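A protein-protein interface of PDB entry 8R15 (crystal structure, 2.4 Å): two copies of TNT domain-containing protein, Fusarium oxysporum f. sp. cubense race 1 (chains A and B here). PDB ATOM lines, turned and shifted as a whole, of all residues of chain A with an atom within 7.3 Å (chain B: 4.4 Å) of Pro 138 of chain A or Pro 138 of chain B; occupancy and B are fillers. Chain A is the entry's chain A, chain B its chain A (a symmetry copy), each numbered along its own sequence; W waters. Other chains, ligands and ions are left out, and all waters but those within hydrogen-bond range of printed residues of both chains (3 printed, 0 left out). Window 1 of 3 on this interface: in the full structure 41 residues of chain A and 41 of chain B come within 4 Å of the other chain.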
ATOM      1  N   LEU A  61      -8.133 -15.805  29.331  1.00  0.00           N
ATOM      2  CA  LEU A  61      -8.989 -16.186  28.209  1.00  0.00           C
ATOM      3  C   LEU A  61     -10.120 -15.180  28.041  1.00  0.00           C
ATOM      4  O   LEU A  61     -10.870 -14.941  28.994  1.00  0.00           O
ATOM      5  CB  LEU A  61      -9.579 -17.565  28.414  1.00  0.00           C
ATOM      6  CG  LEU A  61     -10.446 -18.031  27.247  1.00  0.00           C
ATOM      7  CD1 LEU A  61      -9.583 -18.384  26.053  1.00  0.00           C
ATOM      8  CD2 LEU A  61     -11.315 -19.202  27.649  1.00  0.00           C
ATOM      9  N   PRO A  62     -10.267 -14.558  26.870  1.00  0.00           N
ATOM     10  CA  PRO A  62     -11.428 -13.690  26.626  1.00  0.00           C
ATOM     11  C   PRO A  62     -12.700 -14.524  26.611  1.00  0.00           C
ATOM     12  O   PRO A  62     -12.862 -15.418  25.776  1.00  0.00           O
ATOM     13  CB  PRO A  62     -11.135 -13.076  25.250  1.00  0.00           C
ATOM     14  CG  PRO A  62      -9.665 -13.315  25.021  1.00  0.00           C
ATOM     15  CD  PRO A  62      -9.346 -14.588  25.723  1.00  0.00           C
ATOM     16  N   LEU A  63     -13.608 -14.231  27.530  1.00  0.00           N
ATOM     17  CA  LEU A  63     -14.838 -15.006  27.574  1.00  0.00           C
ATOM     18  C   LEU A  63     -15.932 -14.407  26.704  1.00  0.00           C
ATOM     19  O   LEU A  63     -16.790 -15.144  26.200  1.00  0.00           O
ATOM     20  CB  LEU A  63     -15.326 -15.138  29.018  1.00  0.00           C
ATOM     21  CG  LEU A  63     -14.287 -15.735  29.972  1.00  0.00           C
ATOM     22  CD1 LEU A  63     -14.753 -15.604  31.415  1.00  0.00           C
ATOM     23  CD2 LEU A  63     -13.996 -17.188  29.634  1.00  0.00           C
ATOM     24  N   SER A  64     -15.909 -13.097  26.489  1.00  0.00           N
ATOM     25  CA  SER A  64     -16.957 -12.444  25.720  1.00  0.00           C
ATOM     26  C   SER A  64     -16.421 -11.127  25.180  1.00  0.00           C
ATOM     27  O   SER A  64     -15.243 -10.797  25.337  1.00  0.00           O
ATOM     28  CB  SER A  64     -18.192 -12.206  26.583  1.00  0.00           C
ATOM     29  OG  SER A  64     -17.850 -11.345  27.651  1.00  0.00           O
ATOM     30  N   ALA A  65     -17.303 -10.372  24.541  1.00  0.00           N
ATOM     31  CA  ALA A  65     -17.018  -8.993  24.199  1.00  0.00           C
ATOM     32  C   ALA A  65     -17.636  -8.080  25.255  1.00  0.00           C
ATOM     33  O   ALA A  65     -18.367  -8.524  26.143  1.00  0.00           O
ATOM     34  CB  ALA A  65     -17.541  -8.668  22.803  1.00  0.00           C
ATOM     35  N   TYR A  70     -20.319 -12.379  29.123  1.00  0.00           N
ATOM     36  CA  TYR A  70     -20.475 -13.823  29.137  1.00  0.00           C
ATOM     37  C   TYR A  70     -21.370 -14.240  30.295  1.00  0.00           C
ATOM     38  O   TYR A  70     -21.313 -13.663  31.385  1.00  0.00           O
ATOM     39  CB  TYR A  70     -19.112 -14.498  29.247  1.00  0.00           C
ATOM     40  CG  TYR A  70     -19.173 -16.008  29.355  1.00  0.00           C
ATOM     41  CD1 TYR A  70     -19.453 -16.791  28.245  1.00  0.00           C
ATOM     42  CD2 TYR A  70     -18.923 -16.650  30.566  1.00  0.00           C
ATOM     43  CE1 TYR A  70     -19.495 -18.162  28.336  1.00  0.00           C
ATOM     44  CE2 TYR A  70     -18.965 -18.022  30.665  1.00  0.00           C
ATOM     45  CZ  TYR A  70     -19.251 -18.775  29.548  1.00  0.00           C
ATOM     46  OH  TYR A  70     -19.295 -20.151  29.644  1.00  0.00           O
ATOM     47  N   PHE A 124     -10.296 -26.692  22.315  1.00  0.00           N
ATOM     48  CA  PHE A 124     -10.597 -27.182  23.660  1.00  0.00           C
ATOM     49  C   PHE A 124     -10.742 -28.701  23.559  1.00  0.00           C
ATOM     50  O   PHE A 124     -11.746 -29.202  23.047  1.00  0.00           O
ATOM     51  CB  PHE A 124     -11.864 -26.533  24.219  1.00  0.00           C
ATOM     52  CG  PHE A 124     -11.731 -25.057  24.489  1.00  0.00           C
ATOM     53  CD1 PHE A 124     -12.046 -24.130  23.511  1.00  0.00           C
ATOM     54  CD2 PHE A 124     -11.305 -24.598  25.728  1.00  0.00           C
ATOM     55  CE1 PHE A 124     -11.928 -22.772  23.750  1.00  0.00           C
ATOM     56  CE2 PHE A 124     -11.181 -23.247  25.975  1.00  0.00           C
ATOM     57  CZ  PHE A 124     -11.492 -22.329  24.975  1.00  0.00           C
ATOM     58  N   ALA A 134     -10.719 -20.292  14.992  1.00  0.00           N
ATOM     59  CA  ALA A 134     -10.011 -19.020  14.967  1.00  0.00           C
ATOM     60  C   ALA A 134      -9.748 -18.560  16.392  1.00  0.00           C
ATOM     61  O   ALA A 134     -10.687 -18.356  17.169  1.00  0.00           O
ATOM     62  CB  ALA A 134     -10.823 -17.979  14.200  1.00  0.00           C
ATOM     63  N   ALA A 135      -8.466 -18.421  16.739  1.00  0.00           N
ATOM     64  CA  ALA A 135      -8.082 -18.194  18.127  1.00  0.00           C
ATOM     65  C   ALA A 135      -8.592 -16.866  18.674  1.00  0.00           C
ATOM     66  O   ALA A 135      -8.767 -16.741  19.889  1.00  0.00           O
ATOM     67  CB  ALA A 135      -6.559 -18.266  18.267  1.00  0.00           C
ATOM     68  N   SER A 136      -8.838 -15.876  17.819  1.00  0.00           N
ATOM     69  CA  SER A 136      -9.193 -14.553  18.319  1.00  0.00           C
ATOM     70  C   SER A 136     -10.656 -14.431  18.747  1.00  0.00           C
ATOM     71  O   SER A 136     -11.020 -13.398  19.320  1.00  0.00           O
ATOM     72  CB  SER A 136      -8.860 -13.496  17.266  1.00  0.00           C
ATOM     73  OG  SER A 136      -7.462 -13.430  17.038  1.00  0.00           O
ATOM     74  N   ALA A 137     -11.494 -15.455  18.511  1.00  0.00           N
ATOM     75  CA  ALA A 137     -12.906 -15.397  18.905  1.00  0.00           C
ATOM     76  C   ALA A 137     -13.049 -15.605  20.411  1.00  0.00           C
ATOM     77  O   ALA A 137     -12.475 -16.554  20.960  1.00  0.00           O
ATOM     78  CB  ALA A 137     -13.725 -16.455  18.165  1.00  0.00           C
ATOM     79  N   PRO A 138     -13.804 -14.758  21.106  1.00  0.00           N
ATOM     80  CA  PRO A 138     -14.047 -14.990  22.534  1.00  0.00           C
ATOM     81  C   PRO A 138     -14.820 -16.276  22.779  1.00  0.00           C
ATOM     82  O   PRO A 138     -15.493 -16.817  21.898  1.00  0.00           O
ATOM     83  CB  PRO A 138     -14.864 -13.766  22.960  1.00  0.00           C
ATOM     84  CG  PRO A 138     -15.490 -13.280  21.696  1.00  0.00           C
ATOM     85  CD  PRO A 138     -14.456 -13.522  20.637  1.00  0.00           C
ATOM     86  N   TYR A 139     -14.722 -16.761  24.021  1.00  0.00           N
ATOM     87  CA  TYR A 139     -15.331 -18.043  24.362  1.00  0.00           C
ATOM     88  C   TYR A 139     -16.834 -18.057  24.107  1.00  0.00           C
ATOM     89  O   TYR A 139     -17.402 -19.119  23.829  1.00  0.00           O
ATOM     90  CB  TYR A 139     -15.044 -18.397  25.824  1.00  0.00           C
ATOM     91  CG  TYR A 139     -15.427 -19.813  26.176  1.00  0.00           C
ATOM     92  CD1 TYR A 139     -14.620 -20.873  25.797  1.00  0.00           C
ATOM     93  CD2 TYR A 139     -16.600 -20.094  26.863  1.00  0.00           C
ATOM     94  CE1 TYR A 139     -14.958 -22.176  26.097  1.00  0.00           C
ATOM     95  CE2 TYR A 139     -16.951 -21.404  27.174  1.00  0.00           C
ATOM     96  CZ  TYR A 139     -16.119 -22.440  26.786  1.00  0.00           C
ATOM     97  OH  TYR A 139     -16.436 -23.746  27.081  1.00  0.00           O
ATOM     98  N   SER A 140     -17.497 -16.905  24.212  1.00  0.00           N
ATOM     99  CA  SER A 140     -18.931 -16.861  23.962  1.00  0.00           C
ATOM    100  C   SER A 140     -19.277 -17.221  22.530  1.00  0.00           C
ATOM    101  O   SER A 140     -20.419 -17.603  22.263  1.00  0.00           O
ATOM    102  CB  SER A 140     -19.461 -15.473  24.281  1.00  0.00           C
ATOM    103  OG  SER A 140     -18.877 -14.517  23.422  1.00  0.00           O
ATOM    104  N   GLN A 141     -18.306 -17.157  21.623  1.00  0.00           N
ATOM    105  CA  GLN A 141     -18.524 -17.396  20.207  1.00  0.00           C
ATOM    106  C   GLN A 141     -18.238 -18.823  19.799  1.00  0.00           C
ATOM    107  O   GLN A 141     -18.471 -19.176  18.642  1.00  0.00           O
ATOM    108  CB  GLN A 141     -17.660 -16.456  19.378  1.00  0.00           C
ATOM    109  CG  GLN A 141     -18.173 -15.052  19.376  1.00  0.00           C
ATOM    110  CD  GLN A 141     -17.778 -14.302  18.129  1.00  0.00           C
ATOM    111  OE1 GLN A 141     -16.593 -14.094  17.869  1.00  0.00           O
ATOM    112  NE2 GLN A 141     -18.772 -13.889  17.346  1.00  0.00           N
ATOM    113  N   ARG A 142     -17.730 -19.646  20.700  1.00  0.00           N
ATOM    114  CA  ARG A 142     -17.402 -21.009  20.331  1.00  0.00           C
ATOM    115  C   ARG A 142     -18.537 -21.977  20.594  1.00  0.00           C
ATOM    116  O   ARG A 142     -18.494 -23.103  20.087  1.00  0.00           O
ATOM    117  CB  ARG A 142     -16.139 -21.439  21.064  1.00  0.00           C
ATOM    118  CG  ARG A 142     -14.910 -20.735  20.485  1.00  0.00           C
ATOM    119  CD  ARG A 142     -13.967 -20.291  21.559  1.00  0.00           C
ATOM    120  NE  ARG A 142     -12.976 -19.346  21.059  1.00  0.00           N
ATOM    121  CZ  ARG A 142     -11.853 -19.691  20.448  1.00  0.00           C
ATOM    122  NH1 ARG A 142     -11.581 -20.956  20.162  1.00  0.00           N
ATOM    123  NH2 ARG A 142     -10.985 -18.744  20.107  1.00  0.00           N
ATOM    124  N   ALA A 143     -19.559 -21.552  21.333  1.00  0.00           N
ATOM    125  CA  ALA A 143     -20.735 -22.370  21.599  1.00  0.00           C
ATOM    126  C   ALA A 143     -20.325 -23.708  22.216  1.00  0.00           C
ATOM    127  O   ALA A 143     -20.638 -24.793  21.716  1.00  0.00           O
ATOM    128  CB  ALA A 143     -21.558 -22.562  20.324  1.00  0.00           C
ATOM    129  N   PRO A 185     -23.802 -17.026  22.087  1.00  0.00           N
ATOM    130  CA  PRO A 185     -24.011 -16.435  20.758  1.00  0.00           C
ATOM    131  C   PRO A 185     -23.354 -17.218  19.634  1.00  0.00           C
ATOM    132  O   PRO A 185     -23.872 -17.216  18.508  1.00  0.00           O
ATOM    133  CB  PRO A 185     -23.411 -15.031  20.908  1.00  0.00           C
ATOM    134  CG  PRO A 185     -22.480 -15.136  22.083  1.00  0.00           C
ATOM    135  CD  PRO A 185     -23.135 -16.091  23.007  1.00  0.00           C
ATOM    136  N   GLY A 186     -22.239 -17.893  19.898  1.00  0.00           N
ATOM    137  CA  GLY A 186     -21.606 -18.678  18.849  1.00  0.00           C
ATOM    138  C   GLY A 186     -21.098 -17.787  17.736  1.00  0.00           C
ATOM    139  O   GLY A 186     -20.622 -16.669  17.969  1.00  0.00           O
ATOM    140  N   GLY A 188     -18.541 -17.987  15.932  1.00  0.00           N
ATOM    141  CA  GLY A 188     -17.120 -18.029  15.667  1.00  0.00           C
ATOM    142  C   GLY A 188     -16.831 -18.899  14.455  1.00  0.00           C
ATOM    143  O   GLY A 188     -17.722 -19.464  13.821  1.00  0.00           O
ATOM    144  N   PRO B  62     -13.414  -4.073  21.952  1.00  0.00           N
ATOM    145  CA  PRO B  62     -12.361  -5.101  21.927  1.00  0.00           C
ATOM    146  C   PRO B  62     -11.645  -5.070  20.585  1.00  0.00           C
ATOM    147  O   PRO B  62     -12.254  -5.290  19.535  1.00  0.00           O
ATOM    148  CB  PRO B  62     -13.136  -6.411  22.126  1.00  0.00           C
ATOM    149  CG  PRO B  62     -14.483  -5.992  22.659  1.00  0.00           C
ATOM    150  CD  PRO B  62     -14.759  -4.658  22.062  1.00  0.00           C
ATOM    151  N   LEU B  63     -10.348  -4.801  20.618  1.00  0.00           N
ATOM    152  CA  LEU B  63      -9.614  -4.741  19.364  1.00  0.00           C
ATOM    153  C   LEU B  63      -9.039  -6.091  18.963  1.00  0.00           C
ATOM    154  O   LEU B  63      -8.876  -6.361  17.766  1.00  0.00           O
ATOM    155  CB  LEU B  63      -8.497  -3.699  19.457  1.00  0.00           C
ATOM    156  CG  LEU B  63      -8.982  -2.302  19.855  1.00  0.00           C
ATOM    157  CD1 LEU B  63      -7.800  -1.396  20.164  1.00  0.00           C
ATOM    158  CD2 LEU B  63      -9.855  -1.691  18.771  1.00  0.00           C
ATOM    159  N   SER B  64      -8.754  -6.956  19.929  1.00  0.00           N
ATOM    160  CA  SER B  64      -8.145  -8.242  19.630  1.00  0.00           C
ATOM    161  C   SER B  64      -8.433  -9.202  20.775  1.00  0.00           C
ATOM    162  O   SER B  64      -9.161  -8.882  21.717  1.00  0.00           O
ATOM    163  CB  SER B  64      -6.640  -8.091  19.423  1.00  0.00           C
ATOM    164  OG  SER B  64      -6.056  -7.614  20.619  1.00  0.00           O
ATOM    165  N   SER B 136     -19.827  -9.966  18.817  1.00  0.00           N
ATOM    166  CA  SER B 136     -18.859 -10.401  19.816  1.00  0.00           C
ATOM    167  C   SER B 136     -17.448 -10.601  19.259  1.00  0.00           C
ATOM    168  O   SER B 136     -16.526 -10.825  20.050  1.00  0.00           O
ATOM    169  CB  SER B 136     -19.348 -11.687  20.485  1.00  0.00           C
ATOM    170  OG  SER B 136     -20.540 -11.453  21.218  1.00  0.00           O
ATOM    171  N   ALA B 137     -17.249 -10.501  17.934  1.00  0.00           N
ATOM    172  CA  ALA B 137     -15.918 -10.675  17.343  1.00  0.00           C
ATOM    173  C   ALA B 137     -15.060  -9.434  17.583  1.00  0.00           C
ATOM    174  O   ALA B 137     -15.514  -8.311  17.327  1.00  0.00           O
ATOM    175  CB  ALA B 137     -16.016 -10.943  15.840  1.00  0.00           C
ATOM    176  N   PRO B 138     -13.827  -9.589  18.058  1.00  0.00           N
ATOM    177  CA  PRO B 138     -12.942  -8.427  18.199  1.00  0.00           C
ATOM    178  C   PRO B 138     -12.617  -7.790  16.857  1.00  0.00           C
ATOM    179  O   PRO B 138     -12.741  -8.401  15.792  1.00  0.00           O
ATOM    180  CB  PRO B 138     -11.685  -9.015  18.848  1.00  0.00           C
ATOM    181  CG  PRO B 138     -11.723 -10.462  18.489  1.00  0.00           C
ATOM    182  CD  PRO B 138     -13.178 -10.827  18.520  1.00  0.00           C
ATOM    183  N   TYR B 139     -12.179  -6.529  16.927  1.00  0.00           N
ATOM    184  CA  TYR B 139     -11.930  -5.766  15.708  1.00  0.00           C
ATOM    185  C   TYR B 139     -10.900  -6.438  14.806  1.00  0.00           C
ATOM    186  O   TYR B 139     -10.946  -6.265  13.582  1.00  0.00           O
ATOM    187  CB  TYR B 139     -11.477  -4.345  16.051  1.00  0.00           C
ATOM    188  CG  TYR B 139     -11.441  -3.429  14.852  1.00  0.00           C
ATOM    189  CD1 TYR B 139     -12.612  -2.898  14.340  1.00  0.00           C
ATOM    190  CD2 TYR B 139     -10.246  -3.116  14.219  1.00  0.00           C
ATOM    191  CE1 TYR B 139     -12.604  -2.069  13.236  1.00  0.00           C
ATOM    192  CE2 TYR B 139     -10.223  -2.282  13.107  1.00  0.00           C
ATOM    193  CZ  TYR B 139     -11.411  -1.760  12.625  1.00  0.00           C
ATOM    194  OH  TYR B 139     -11.422  -0.928  11.529  1.00  0.00           O
ATOM    195  N   SER B 140      -9.959  -7.187  15.380  1.00  0.00           N
ATOM    196  CA  SER B 140      -8.961  -7.865  14.562  1.00  0.00           C
ATOM    197  C   SER B 140      -9.580  -8.897  13.638  1.00  0.00           C
ATOM    198  O   SER B 140      -8.954  -9.264  12.640  1.00  0.00           O
ATOM    199  CB  SER B 140      -7.935  -8.532  15.459  1.00  0.00           C
ATOM    200  OG  SER B 140      -8.547  -9.530  16.247  1.00  0.00           O
ATOM    201  N   GLN B 141     -10.805  -9.330  13.923  1.00  0.00           N
ATOM    202  CA  GLN B 141     -11.475 -10.374  13.169  1.00  0.00           C
ATOM    203  C   GLN B 141     -12.373  -9.833  12.080  1.00  0.00           C
ATOM    204  O   GLN B 141     -12.927 -10.619  11.311  1.00  0.00           O
ATOM    205  CB  GLN B 141     -12.296 -11.252  14.104  1.00  0.00           C
ATOM    206  CG  GLN B 141     -11.447 -12.173  14.922  1.00  0.00           C
ATOM    207  CD  GLN B 141     -12.189 -13.423  15.324  1.00  0.00           C
ATOM    208  OE1 GLN B 141     -13.186 -13.360  16.042  1.00  0.00           O
ATOM    209  NE2 GLN B 141     -11.705 -14.574  14.862  1.00  0.00           N
ATOM    210  N   ARG B 142     -12.545  -8.525  11.999  1.00  0.00           N
ATOM    211  CA  ARG B 142     -13.434  -7.975  10.996  1.00  0.00           C
ATOM    212  C   ARG B 142     -12.717  -7.609   9.713  1.00  0.00           C
ATOM    213  O   ARG B 142     -13.382  -7.385   8.697  1.00  0.00           O
ATOM    214  CB  ARG B 142     -14.161  -6.768  11.575  1.00  0.00           C
ATOM    215  CG  ARG B 142     -15.207  -7.206  12.601  1.00  0.00           C
ATOM    216  CD  ARG B 142     -15.221  -6.307  13.798  1.00  0.00           C
ATOM    217  NE  ARG B 142     -15.960  -6.890  14.911  1.00  0.00           N
ATOM    218  CZ  ARG B 142     -17.277  -6.823  15.052  1.00  0.00           C
ATOM    219  NH1 ARG B 142     -18.045  -6.277  14.122  1.00  0.00           N
ATOM    220  NH2 ARG B 142     -17.835  -7.321  16.151  1.00  0.00           N
HETATM  221  O   HOH W   1     -19.637 -12.011  23.721  1.00  0.00           O
HETATM  222  O   HOH W   2     -15.379 -14.436  15.758  1.00  0.00           O
HETATM  223  O   HOH W   3      -6.994 -10.889  17.886  1.00  0.00           O
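O of Ala 134 of chain A sits at hydrogen-bond distance from NH2 of Arg 142 of chain A (3.0 Å).
The backbone carbonyl oxygen (O) of Ala 137 of chain A is in hydrogen-bond range of the guanidinium group (NH2) of Arg 142 of chain A, 2.8 Å away.
The backbone carbonyl oxygen of Gly 186 of chain A sits close to the side-chain amide nitrogen of Gln 141 of chain A, at 3.4 Å.
The backbone carbonyl oxygen of Gln 141 of chain A is in hydrogen-bond range of the backbone NH of Gly 188 of chain A, at 3.0 Å.
O of Ala 137 of chain B is in hydrogen-bond range of NH2 of Arg 142 of chain B (2.8 Å).
Ser 64 of chain A touches none of the printed residues of chain B.
Printed residues of chain B within 4 Å of Ala 65 of chain A: Ser 136.
Phe 124 of chain A touches none of the printed residues of chain B.
Printed residues of chain B within 4 Å of Ala 137 of chain A: Gln 141 (3.5 Å).
Pro 138 of chain A touches two residues of chain B.
Of the printed residues of chain B, Gln 141 of chain A touches Ser 136, Ala 137 and Gln 141.
Of the printed residues of chain A, Ser 136 of chain B touches Ala 65 (3.6 Å), Pro 138 (3.1 Å) and Gln 141 (3.7 Å).
Pro 138 of chain B touches two residues of chain A.
The nearest printed residue of chain B that does not touch Pro 138 of chain A is Ala 137 of chain B (4.6 Å).
Ser 136 of chain A touches Pro 138 of chain B, and with the chains exchanged Pro 138 of chain A touches Ser 136 of chain B.
Ser 136 of chain A touches Gln 141 of chain B, and with the chains exchanged Gln 141 of chain A touches Ser 136 of chain B.
Ala 137 of chain A touches Gln 141 of chain B, and with the chains exchanged Gln 141 of chain A touches Ala 137 of chain B.
Gln 141 of chain A touches its own counterpart, Gln 141 of chain B.
Of the 10 pairs that touch across the chains among the printed residues, 8 have their exchanged pair printed and touching as well.
Water W2 lies within hydrogen-bond range of OE1 of Gln 141 of chain A (2.5 Å) and OE1 of Gln 141 of chain B (2.5 Å).
Water W3 lies within hydrogen-bond range of the side-chain hydroxyl (OG) of Ser 140 of chain B (2.6 Å) and the side-chain hydroxyl (OG) of Ser 136 of chain A (2.7 Å).
Water W1 lies within hydrogen-bond range of the side-chain hydroxyl (OG) of Ser 140 of chain A (2.6 Å), the side-chain hydroxyl (OG) of Ser 136 of chain B (2.7 Å) and the backbone NH (N) of Ala 65 of chain A (3.0 Å).
CB of Ala 65 of chain A touches O of Ser 136 of chain B, at 3.6 Å.
NE2 of Gln 141 of chain B touches CB of Ala 134 of chain A (3.6 Å).
Ser 136 of chain A touches Pro 138 of chain B.
Ser 136 of chain A touches Gln 141 of chain B.
Ala 137 of chain A touches Gln 141 of chain B (CA to OE1, 3.5 Å).
Pro 138 of chain A touches Ser 136 of chain B.
Pro 138 of chain A touches Pro 138 of chain B (CD to CD, 3.7 Å).
Ser 136 of chain B touches Gln 141 of chain A.
CA of Ala 137 of chain B touches OE1 of Gln 141 of chain A, 3.5 Å away.
Gln 141 of chain A touches Gln 141 of chain B.
Of the 20 printed residues of chain A, 6 touch a printed residue of chain B.
Hydrophobic or aromatic side chains of chain A that line the printed part of chain B: Ala 65, Ala 134, Ala 137 and Pro 138.
Among the printed residues, no Asp or Glu carboxylate lies within 4 Å of a Lys or Arg side-chain nitrogen of the other chain.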
